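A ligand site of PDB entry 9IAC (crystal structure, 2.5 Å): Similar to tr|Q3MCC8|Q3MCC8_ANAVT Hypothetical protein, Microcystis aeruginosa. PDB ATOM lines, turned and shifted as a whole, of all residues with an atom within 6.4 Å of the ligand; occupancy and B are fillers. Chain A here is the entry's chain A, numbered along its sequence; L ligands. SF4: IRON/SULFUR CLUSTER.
An iron atom (FE4) of the ligand is bound by the side-chain sulfur (SG) of Cys 264. A sulfur (S3) of the ligand sits close to the backbone NH (N) of Lys 37, 3.8 Å away. An iron atom (FE1) of the ligand is bound by the side-chain sulfur (SG) of Cys 270, at 2.2 Å. The side-chain sulfur (SG) of Cys 34 binds an iron atom (FE2) of the ligand. The side-chain sulfur of Cys 261 is bound to an iron atom (FE3) of the ligand (2.2 Å).
SG of Cys 34 lies close to N of Thr 36. SG of Cys 264 sits close to N of Phe 266, 3.3 Å away. The backbone carbonyl oxygen of Cys 264 lies within hydrogen-bond range of the side-chain hydroxyl of Thr 267 (3.1 Å). O of Cys 261 lies within hydrogen-bond range of OG1 of Thr 267, at 2.4 Å. N of Gln 256 lies close to SG of Cys 34 (3.6 Å). The side-chain sulfur of Cys 261 lies close to the backbone NH of Gly 258. SG of Cys 270 sits close to N of Tyr 272.
Residues that only touch the ligand: Thr 36 (3.9 Å), Gln 256 (3.9 Å), Thr 267 (3.95 Å) and Ala 273 (3.8 Å). Hydrophobic or aromatic side chains that line the ligand: Ala 273. Nine residues have an atom within 4 Å of the ligand: Cys 34, Thr 36, Lys 37, Gln 256, Cys 261, Cys 264, Thr 267, Cys 270 and Ala 273. The nearest printed residue that does not touch the ligand is Ser 257 (4.02 Å).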
ATOM      1  N   CYS A  34     -23.509   5.482 -21.816  1.00  0.00           N
ATOM      2  CA  CYS A  34     -23.939   6.884 -21.889  1.00  0.00           C
ATOM      3  C   CYS A  34     -24.741   7.230 -20.642  1.00  0.00           C
ATOM      4  O   CYS A  34     -25.834   6.700 -20.429  1.00  0.00           O
ATOM      5  CB  CYS A  34     -24.756   7.149 -23.150  1.00  0.00           C
ATOM      6  SG  CYS A  34     -25.357   8.855 -23.269  1.00  0.00           S
ATOM      7  N   GLN A  35     -24.196   8.140 -19.818  1.00  0.00           N
ATOM      8  CA  GLN A  35     -24.856   8.544 -18.590  1.00  0.00           C
ATOM      9  C   GLN A  35     -26.224   9.183 -18.859  1.00  0.00           C
ATOM     10  O   GLN A  35     -27.126   9.096 -18.015  1.00  0.00           O
ATOM     11  CB  GLN A  35     -23.961   9.516 -17.812  1.00  0.00           C
ATOM     12  CG  GLN A  35     -22.636   8.916 -17.362  1.00  0.00           C
ATOM     13  CD  GLN A  35     -21.915   9.794 -16.369  1.00  0.00           C
ATOM     14  OE1 GLN A  35     -22.511  10.285 -15.406  1.00  0.00           O
ATOM     15  NE2 GLN A  35     -20.627   9.999 -16.589  1.00  0.00           N
ATOM     16  N   THR A  36     -26.387   9.832 -20.007  1.00  0.00           N
ATOM     17  CA  THR A  36     -27.674  10.418 -20.352  1.00  0.00           C
ATOM     18  C   THR A  36     -28.745   9.354 -20.500  1.00  0.00           C
ATOM     19  O   THR A  36     -29.931   9.615 -20.255  1.00  0.00           O
ATOM     20  CB  THR A  36     -27.549  11.233 -21.637  1.00  0.00           C
ATOM     21  OG1 THR A  36     -26.332  11.968 -21.597  1.00  0.00           O
ATOM     22  CG2 THR A  36     -28.707  12.206 -21.764  1.00  0.00           C
ATOM     23  N   LYS A  37     -28.358   8.138 -20.898  1.00  0.00           N
ATOM     24  CA  LYS A  37     -29.333   7.061 -20.941  1.00  0.00           C
ATOM     25  C   LYS A  37     -29.859   6.753 -19.534  1.00  0.00           C
ATOM     26  O   LYS A  37     -31.061   6.536 -19.358  1.00  0.00           O
ATOM     27  CB  LYS A  37     -28.695   5.821 -21.568  1.00  0.00           C
ATOM     28  CG  LYS A  37     -29.636   4.651 -21.723  1.00  0.00           C
ATOM     29  CD  LYS A  37     -28.899   3.482 -22.357  1.00  0.00           C
ATOM     30  CE  LYS A  37     -29.732   2.218 -22.350  1.00  0.00           C
ATOM     31  NZ  LYS A  37     -28.971   1.069 -22.889  1.00  0.00           N
ATOM     32  N   ARG A  38     -28.972   6.750 -18.543  1.00  0.00           N
ATOM     33  CA  ARG A  38     -29.421   6.615 -17.152  1.00  0.00           C
ATOM     34  C   ARG A  38     -30.267   7.814 -16.735  1.00  0.00           C
ATOM     35  O   ARG A  38     -31.207   7.675 -15.947  1.00  0.00           O
ATOM     36  CB  ARG A  38     -28.216   6.437 -16.240  1.00  0.00           C
ATOM     37  CG  ARG A  38     -28.561   6.320 -14.756  1.00  0.00           C
ATOM     38  CD  ARG A  38     -27.331   6.007 -13.923  1.00  0.00           C
ATOM     39  NE  ARG A  38     -26.200   6.863 -14.273  1.00  0.00           N
ATOM     40  CZ  ARG A  38     -25.967   8.045 -13.709  1.00  0.00           C
ATOM     41  NH1 ARG A  38     -26.732   8.526 -12.746  1.00  0.00           N
ATOM     42  NH2 ARG A  38     -24.937   8.773 -14.134  1.00  0.00           N
ATOM     43  N   PHE A  40     -32.297   9.346 -18.585  1.00  0.00           N
ATOM     44  CA  PHE A  40     -33.641   9.118 -19.119  1.00  0.00           C
ATOM     45  C   PHE A  40     -34.360   7.984 -18.397  1.00  0.00           C
ATOM     46  O   PHE A  40     -35.560   8.074 -18.148  1.00  0.00           O
ATOM     47  CB  PHE A  40     -33.577   8.810 -20.615  1.00  0.00           C
ATOM     48  CG  PHE A  40     -33.533  10.029 -21.494  1.00  0.00           C
ATOM     49  CD1 PHE A  40     -34.580  10.944 -21.485  1.00  0.00           C
ATOM     50  CD2 PHE A  40     -32.454  10.249 -22.330  1.00  0.00           C
ATOM     51  CE1 PHE A  40     -34.541  12.058 -22.297  1.00  0.00           C
ATOM     52  CE2 PHE A  40     -32.415  11.363 -23.142  1.00  0.00           C
ATOM     53  CZ  PHE A  40     -33.458  12.267 -23.125  1.00  0.00           C
ATOM     54  N   TYR A 250     -28.302  17.674 -19.449  1.00  0.00           N
ATOM     55  CA  TYR A 250     -27.184  17.077 -20.150  1.00  0.00           C
ATOM     56  C   TYR A 250     -25.839  17.374 -19.503  1.00  0.00           C
ATOM     57  O   TYR A 250     -24.835  16.754 -19.876  1.00  0.00           O
ATOM     58  CB  TYR A 250     -27.192  17.516 -21.610  1.00  0.00           C
ATOM     59  CG  TYR A 250     -28.428  17.077 -22.359  1.00  0.00           C
ATOM     60  CD1 TYR A 250     -28.529  15.795 -22.872  1.00  0.00           C
ATOM     61  CD2 TYR A 250     -29.496  17.940 -22.533  1.00  0.00           C
ATOM     62  CE1 TYR A 250     -29.661  15.386 -23.549  1.00  0.00           C
ATOM     63  CE2 TYR A 250     -30.631  17.542 -23.218  1.00  0.00           C
ATOM     64  CZ  TYR A 250     -30.709  16.263 -23.724  1.00  0.00           C
ATOM     65  OH  TYR A 250     -31.841  15.876 -24.393  1.00  0.00           O
ATOM     66  N   PRO A 255     -23.587  13.307 -21.953  1.00  0.00           N
ATOM     67  CA  PRO A 255     -23.716  12.371 -23.072  1.00  0.00           C
ATOM     68  C   PRO A 255     -22.380  11.894 -23.623  1.00  0.00           C
ATOM     69  O   PRO A 255     -21.368  12.591 -23.594  1.00  0.00           O
ATOM     70  CB  PRO A 255     -24.474  13.189 -24.125  1.00  0.00           C
ATOM     71  CG  PRO A 255     -24.080  14.609 -23.831  1.00  0.00           C
ATOM     72  CD  PRO A 255     -23.889  14.699 -22.344  1.00  0.00           C
ATOM     73  N   GLN A 256     -22.392  10.658 -24.111  1.00  0.00           N
ATOM     74  CA  GLN A 256     -21.317  10.115 -24.945  1.00  0.00           C
ATOM     75  C   GLN A 256     -21.975   9.644 -26.240  1.00  0.00           C
ATOM     76  O   GLN A 256     -22.659   8.621 -26.249  1.00  0.00           O
ATOM     77  CB  GLN A 256     -20.570   8.986 -24.237  1.00  0.00           C
ATOM     78  CG  GLN A 256     -19.223   8.627 -24.853  1.00  0.00           C
ATOM     79  CD  GLN A 256     -18.640   7.373 -24.237  1.00  0.00           C
ATOM     80  OE1 GLN A 256     -19.374   6.518 -23.733  1.00  0.00           O
ATOM     81  NE2 GLN A 256     -17.321   7.260 -24.251  1.00  0.00           N
ATOM     82  N   SER A 257     -21.769  10.403 -27.309  1.00  0.00           N
ATOM     83  CA  SER A 257     -22.496  10.225 -28.558  1.00  0.00           C
ATOM     84  C   SER A 257     -21.727   9.349 -29.530  1.00  0.00           C
ATOM     85  O   SER A 257     -20.563   8.992 -29.309  1.00  0.00           O
ATOM     86  CB  SER A 257     -22.793  11.591 -29.183  1.00  0.00           C
ATOM     87  OG  SER A 257     -23.404  12.447 -28.238  1.00  0.00           O
ATOM     88  N   GLY A 258     -22.401   8.978 -30.620  1.00  0.00           N
ATOM     89  CA  GLY A 258     -21.783   8.159 -31.657  1.00  0.00           C
ATOM     90  C   GLY A 258     -22.717   7.140 -32.280  1.00  0.00           C
ATOM     91  O   GLY A 258     -23.941   7.281 -32.204  1.00  0.00           O
ATOM     92  N   VAL A 260     -23.298   4.089 -31.363  1.00  0.00           N
ATOM     93  CA  VAL A 260     -24.055   3.395 -30.332  1.00  0.00           C
ATOM     94  C   VAL A 260     -25.334   4.144 -29.980  1.00  0.00           C
ATOM     95  O   VAL A 260     -26.202   3.591 -29.286  1.00  0.00           O
ATOM     96  CB  VAL A 260     -23.163   3.192 -29.093  1.00  0.00           C
ATOM     97  CG1 VAL A 260     -23.804   2.234 -28.087  1.00  0.00           C
ATOM     98  CG2 VAL A 260     -21.795   2.676 -29.520  1.00  0.00           C
ATOM     99  N   CYS A 261     -25.483   5.375 -30.456  1.00  0.00           N
ATOM    100  CA  CYS A 261     -26.720   6.113 -30.255  1.00  0.00           C
ATOM    101  C   CYS A 261     -27.804   5.737 -31.255  1.00  0.00           C
ATOM    102  O   CYS A 261     -28.899   6.296 -31.186  1.00  0.00           O
ATOM    103  CB  CYS A 261     -26.456   7.614 -30.312  1.00  0.00           C
ATOM    104  SG  CYS A 261     -25.242   8.191 -29.095  1.00  0.00           S
ATOM    105  N   ARG A 262     -27.516   4.828 -32.191  1.00  0.00           N
ATOM    106  CA  ARG A 262     -28.544   4.242 -33.032  1.00  0.00           C
ATOM    107  C   ARG A 262     -29.245   3.087 -32.335  1.00  0.00           C
ATOM    108  O   ARG A 262     -30.200   2.542 -32.891  1.00  0.00           O
ATOM    109  CB  ARG A 262     -27.958   3.748 -34.356  1.00  0.00           C
ATOM    110  CG  ARG A 262     -27.207   4.799 -35.161  1.00  0.00           C
ATOM    111  CD  ARG A 262     -26.681   4.187 -36.462  1.00  0.00           C
ATOM    112  NE  ARG A 262     -25.823   5.094 -37.217  1.00  0.00           N
ATOM    113  CZ  ARG A 262     -25.224   4.785 -38.354  1.00  0.00           C
ATOM    114  NH1 ARG A 262     -25.385   3.590 -38.908  1.00  0.00           N
ATOM    115  NH2 ARG A 262     -24.456   5.680 -38.958  1.00  0.00           N
ATOM    116  N   TYR A 263     -28.788   2.714 -31.143  1.00  0.00           N
ATOM    117  CA  TYR A 263     -29.376   1.619 -30.385  1.00  0.00           C
ATOM    118  C   TYR A 263     -30.022   2.094 -29.099  1.00  0.00           C
ATOM    119  O   TYR A 263     -30.659   1.285 -28.407  1.00  0.00           O
ATOM    120  CB  TYR A 263     -28.310   0.563 -30.066  1.00  0.00           C
ATOM    121  CG  TYR A 263     -27.731  -0.096 -31.304  1.00  0.00           C
ATOM    122  CD1 TYR A 263     -28.190  -1.331 -31.725  1.00  0.00           C
ATOM    123  CD2 TYR A 263     -26.742   0.531 -32.037  1.00  0.00           C
ATOM    124  CE1 TYR A 263     -27.673  -1.935 -32.867  1.00  0.00           C
ATOM    125  CE2 TYR A 263     -26.219  -0.061 -33.177  1.00  0.00           C
ATOM    126  CZ  TYR A 263     -26.681  -1.296 -33.584  1.00  0.00           C
ATOM    127  OH  TYR A 263     -26.168  -1.901 -34.712  1.00  0.00           O
ATOM    128  N   CYS A 264     -29.886   3.365 -28.760  1.00  0.00           N
ATOM    129  CA  CYS A 264     -30.518   3.890 -27.564  1.00  0.00           C
ATOM    130  C   CYS A 264     -32.032   3.870 -27.731  1.00  0.00           C
ATOM    131  O   CYS A 264     -32.548   4.188 -28.808  1.00  0.00           O
ATOM    132  CB  CYS A 264     -30.049   5.314 -27.285  1.00  0.00           C
ATOM    133  SG  CYS A 264     -30.625   5.935 -25.705  1.00  0.00           S
ATOM    134  N   PRO A 265     -32.777   3.497 -26.689  1.00  0.00           N
ATOM    135  CA  PRO A 265     -34.241   3.639 -26.734  1.00  0.00           C
ATOM    136  C   PRO A 265     -34.682   5.086 -26.852  1.00  0.00           C
ATOM    137  O   PRO A 265     -35.870   5.329 -27.135  1.00  0.00           O
ATOM    138  CB  PRO A 265     -34.692   3.033 -25.408  1.00  0.00           C
ATOM    139  CG  PRO A 265     -33.564   2.158 -24.970  1.00  0.00           C
ATOM    140  CD  PRO A 265     -32.327   2.837 -25.446  1.00  0.00           C
ATOM    141  N   PHE A 266     -33.767   6.049 -26.676  1.00  0.00           N
ATOM    142  CA  PHE A 266     -34.121   7.459 -26.605  1.00  0.00           C
ATOM    143  C   PHE A 266     -33.580   8.272 -27.774  1.00  0.00           C
ATOM    144  O   PHE A 266     -33.610   9.507 -27.707  1.00  0.00           O
ATOM    145  CB  PHE A 266     -33.621   8.055 -25.287  1.00  0.00           C
ATOM    146  CG  PHE A 266     -33.906   7.186 -24.096  1.00  0.00           C
ATOM    147  CD1 PHE A 266     -35.194   6.985 -23.664  1.00  0.00           C
ATOM    148  CD2 PHE A 266     -32.863   6.578 -23.413  1.00  0.00           C
ATOM    149  CE1 PHE A 266     -35.456   6.178 -22.575  1.00  0.00           C
ATOM    150  CE2 PHE A 266     -33.124   5.771 -22.324  1.00  0.00           C
ATOM    151  CZ  PHE A 266     -34.418   5.574 -21.908  1.00  0.00           C
ATOM    152  N   THR A 267     -33.107   7.639 -28.849  1.00  0.00           N
ATOM    153  CA  THR A 267     -32.517   8.376 -29.958  1.00  0.00           C
ATOM    154  C   THR A 267     -33.452   9.457 -30.483  1.00  0.00           C
ATOM    155  O   THR A 267     -33.000  10.525 -30.919  1.00  0.00           O
ATOM    156  CB  THR A 267     -32.134   7.412 -31.085  1.00  0.00           C
ATOM    157  OG1 THR A 267     -31.239   6.420 -30.581  1.00  0.00           O
ATOM    158  CG2 THR A 267     -31.458   8.144 -32.230  1.00  0.00           C
ATOM    159  N   SER A 268     -34.758   9.210 -30.430  1.00  0.00           N
ATOM    160  CA  SER A 268     -35.741  10.163 -30.952  1.00  0.00           C
ATOM    161  C   SER A 268     -35.847  11.427 -30.098  1.00  0.00           C
ATOM    162  O   SER A 268     -36.330  12.447 -30.596  1.00  0.00           O
ATOM    163  CB  SER A 268     -37.117   9.496 -31.052  1.00  0.00           C
ATOM    164  OG  SER A 268     -38.152  10.454 -31.089  1.00  0.00           O
ATOM    165  N   CYS A 270     -33.164  12.450 -27.713  1.00  0.00           N
ATOM    166  CA  CYS A 270     -31.877  12.874 -27.164  1.00  0.00           C
ATOM    167  C   CYS A 270     -31.244  13.918 -28.081  1.00  0.00           C
ATOM    168  O   CYS A 270     -30.993  13.642 -29.255  1.00  0.00           O
ATOM    169  CB  CYS A 270     -30.917  11.701 -26.965  1.00  0.00           C
ATOM    170  SG  CYS A 270     -29.307  12.200 -26.277  1.00  0.00           S
ATOM    171  N   ASP A 271     -30.995  15.102 -27.534  1.00  0.00           N
ATOM    172  CA  ASP A 271     -30.450  16.215 -28.309  1.00  0.00           C
ATOM    173  C   ASP A 271     -29.027  15.968 -28.784  1.00  0.00           C
ATOM    174  O   ASP A 271     -28.572  16.646 -29.712  1.00  0.00           O
ATOM    175  CB  ASP A 271     -30.510  17.490 -27.473  1.00  0.00           C
ATOM    176  CG  ASP A 271     -31.914  18.069 -27.388  1.00  0.00           C
ATOM    177  OD1 ASP A 271     -32.852  17.438 -27.922  1.00  0.00           O
ATOM    178  OD2 ASP A 271     -32.073  19.148 -26.791  1.00  0.00           O
ATOM    179  N   TYR A 272     -28.304  15.023 -28.184  1.00  0.00           N
ATOM    180  CA  TYR A 272     -26.943  14.710 -28.598  1.00  0.00           C
ATOM    181  C   TYR A 272     -26.860  13.414 -29.385  1.00  0.00           C
ATOM    182  O   TYR A 272     -25.766  12.884 -29.577  1.00  0.00           O
ATOM    183  CB  TYR A 272     -26.009  14.635 -27.386  1.00  0.00           C
ATOM    184  CG  TYR A 272     -25.805  15.969 -26.691  1.00  0.00           C
ATOM    185  CD1 TYR A 272     -26.755  16.474 -25.826  1.00  0.00           C
ATOM    186  CD2 TYR A 272     -24.655  16.721 -26.916  1.00  0.00           C
ATOM    187  CE1 TYR A 272     -26.577  17.689 -25.201  1.00  0.00           C
ATOM    188  CE2 TYR A 272     -24.472  17.943 -26.297  1.00  0.00           C
ATOM    189  CZ  TYR A 272     -25.436  18.423 -25.436  1.00  0.00           C
ATOM    190  OH  TYR A 272     -25.250  19.627 -24.817  1.00  0.00           O
ATOM    191  N   ALA A 273     -27.998  12.885 -29.820  1.00  0.00           N
ATOM    192  CA  ALA A 273     -27.996  11.654 -30.604  1.00  0.00           C
ATOM    193  C   ALA A 273     -27.213  11.847 -31.884  1.00  0.00           C
ATOM    194  O   ALA A 273     -27.396  12.832 -32.598  1.00  0.00           O
ATOM    195  CB  ALA A 273     -29.431  11.231 -30.914  1.00  0.00           C
ATOM    196  N   ASN A 274     -26.314  10.904 -32.174  1.00  0.00           N
ATOM    197  CA  ASN A 274     -25.617  10.901 -33.455  1.00  0.00           C
ATOM    198  C   ASN A 274     -26.553  10.310 -34.498  1.00  0.00           C
ATOM    199  O   ASN A 274     -26.998   9.165 -34.371  1.00  0.00           O
ATOM    200  CB  ASN A 274     -24.315  10.109 -33.363  1.00  0.00           C
ATOM    201  CG  ASN A 274     -23.361  10.387 -34.523  1.00  0.00           C
ATOM    202  OD1 ASN A 274     -23.630  11.252 -35.359  1.00  0.00           O
ATOM    203  ND2 ASN A 274     -22.244   9.673 -34.556  1.00  0.00           N
HETATM  204 FE1  SF4 L   1     -28.487  10.151 -26.409  1.00  0.00          FE
HETATM  205 FE2  SF4 L   1     -26.811   8.613 -24.907  1.00  0.00          FE
HETATM  206 FE3  SF4 L   1     -26.840   8.352 -27.631  1.00  0.00          FE
HETATM  207 FE4  SF4 L   1     -28.968   7.481 -26.159  1.00  0.00          FE
HETATM  208  S1  SF4 L   1     -26.831   6.650 -26.086  1.00  0.00           S
HETATM  209  S2  SF4 L   1     -29.051   8.701 -28.087  1.00  0.00           S
HETATM  210  S3  SF4 L   1     -29.020   9.040 -24.489  1.00  0.00           S
HETATM  211  S4  SF4 L   1     -26.212  10.194 -26.445  1.00  0.00           S
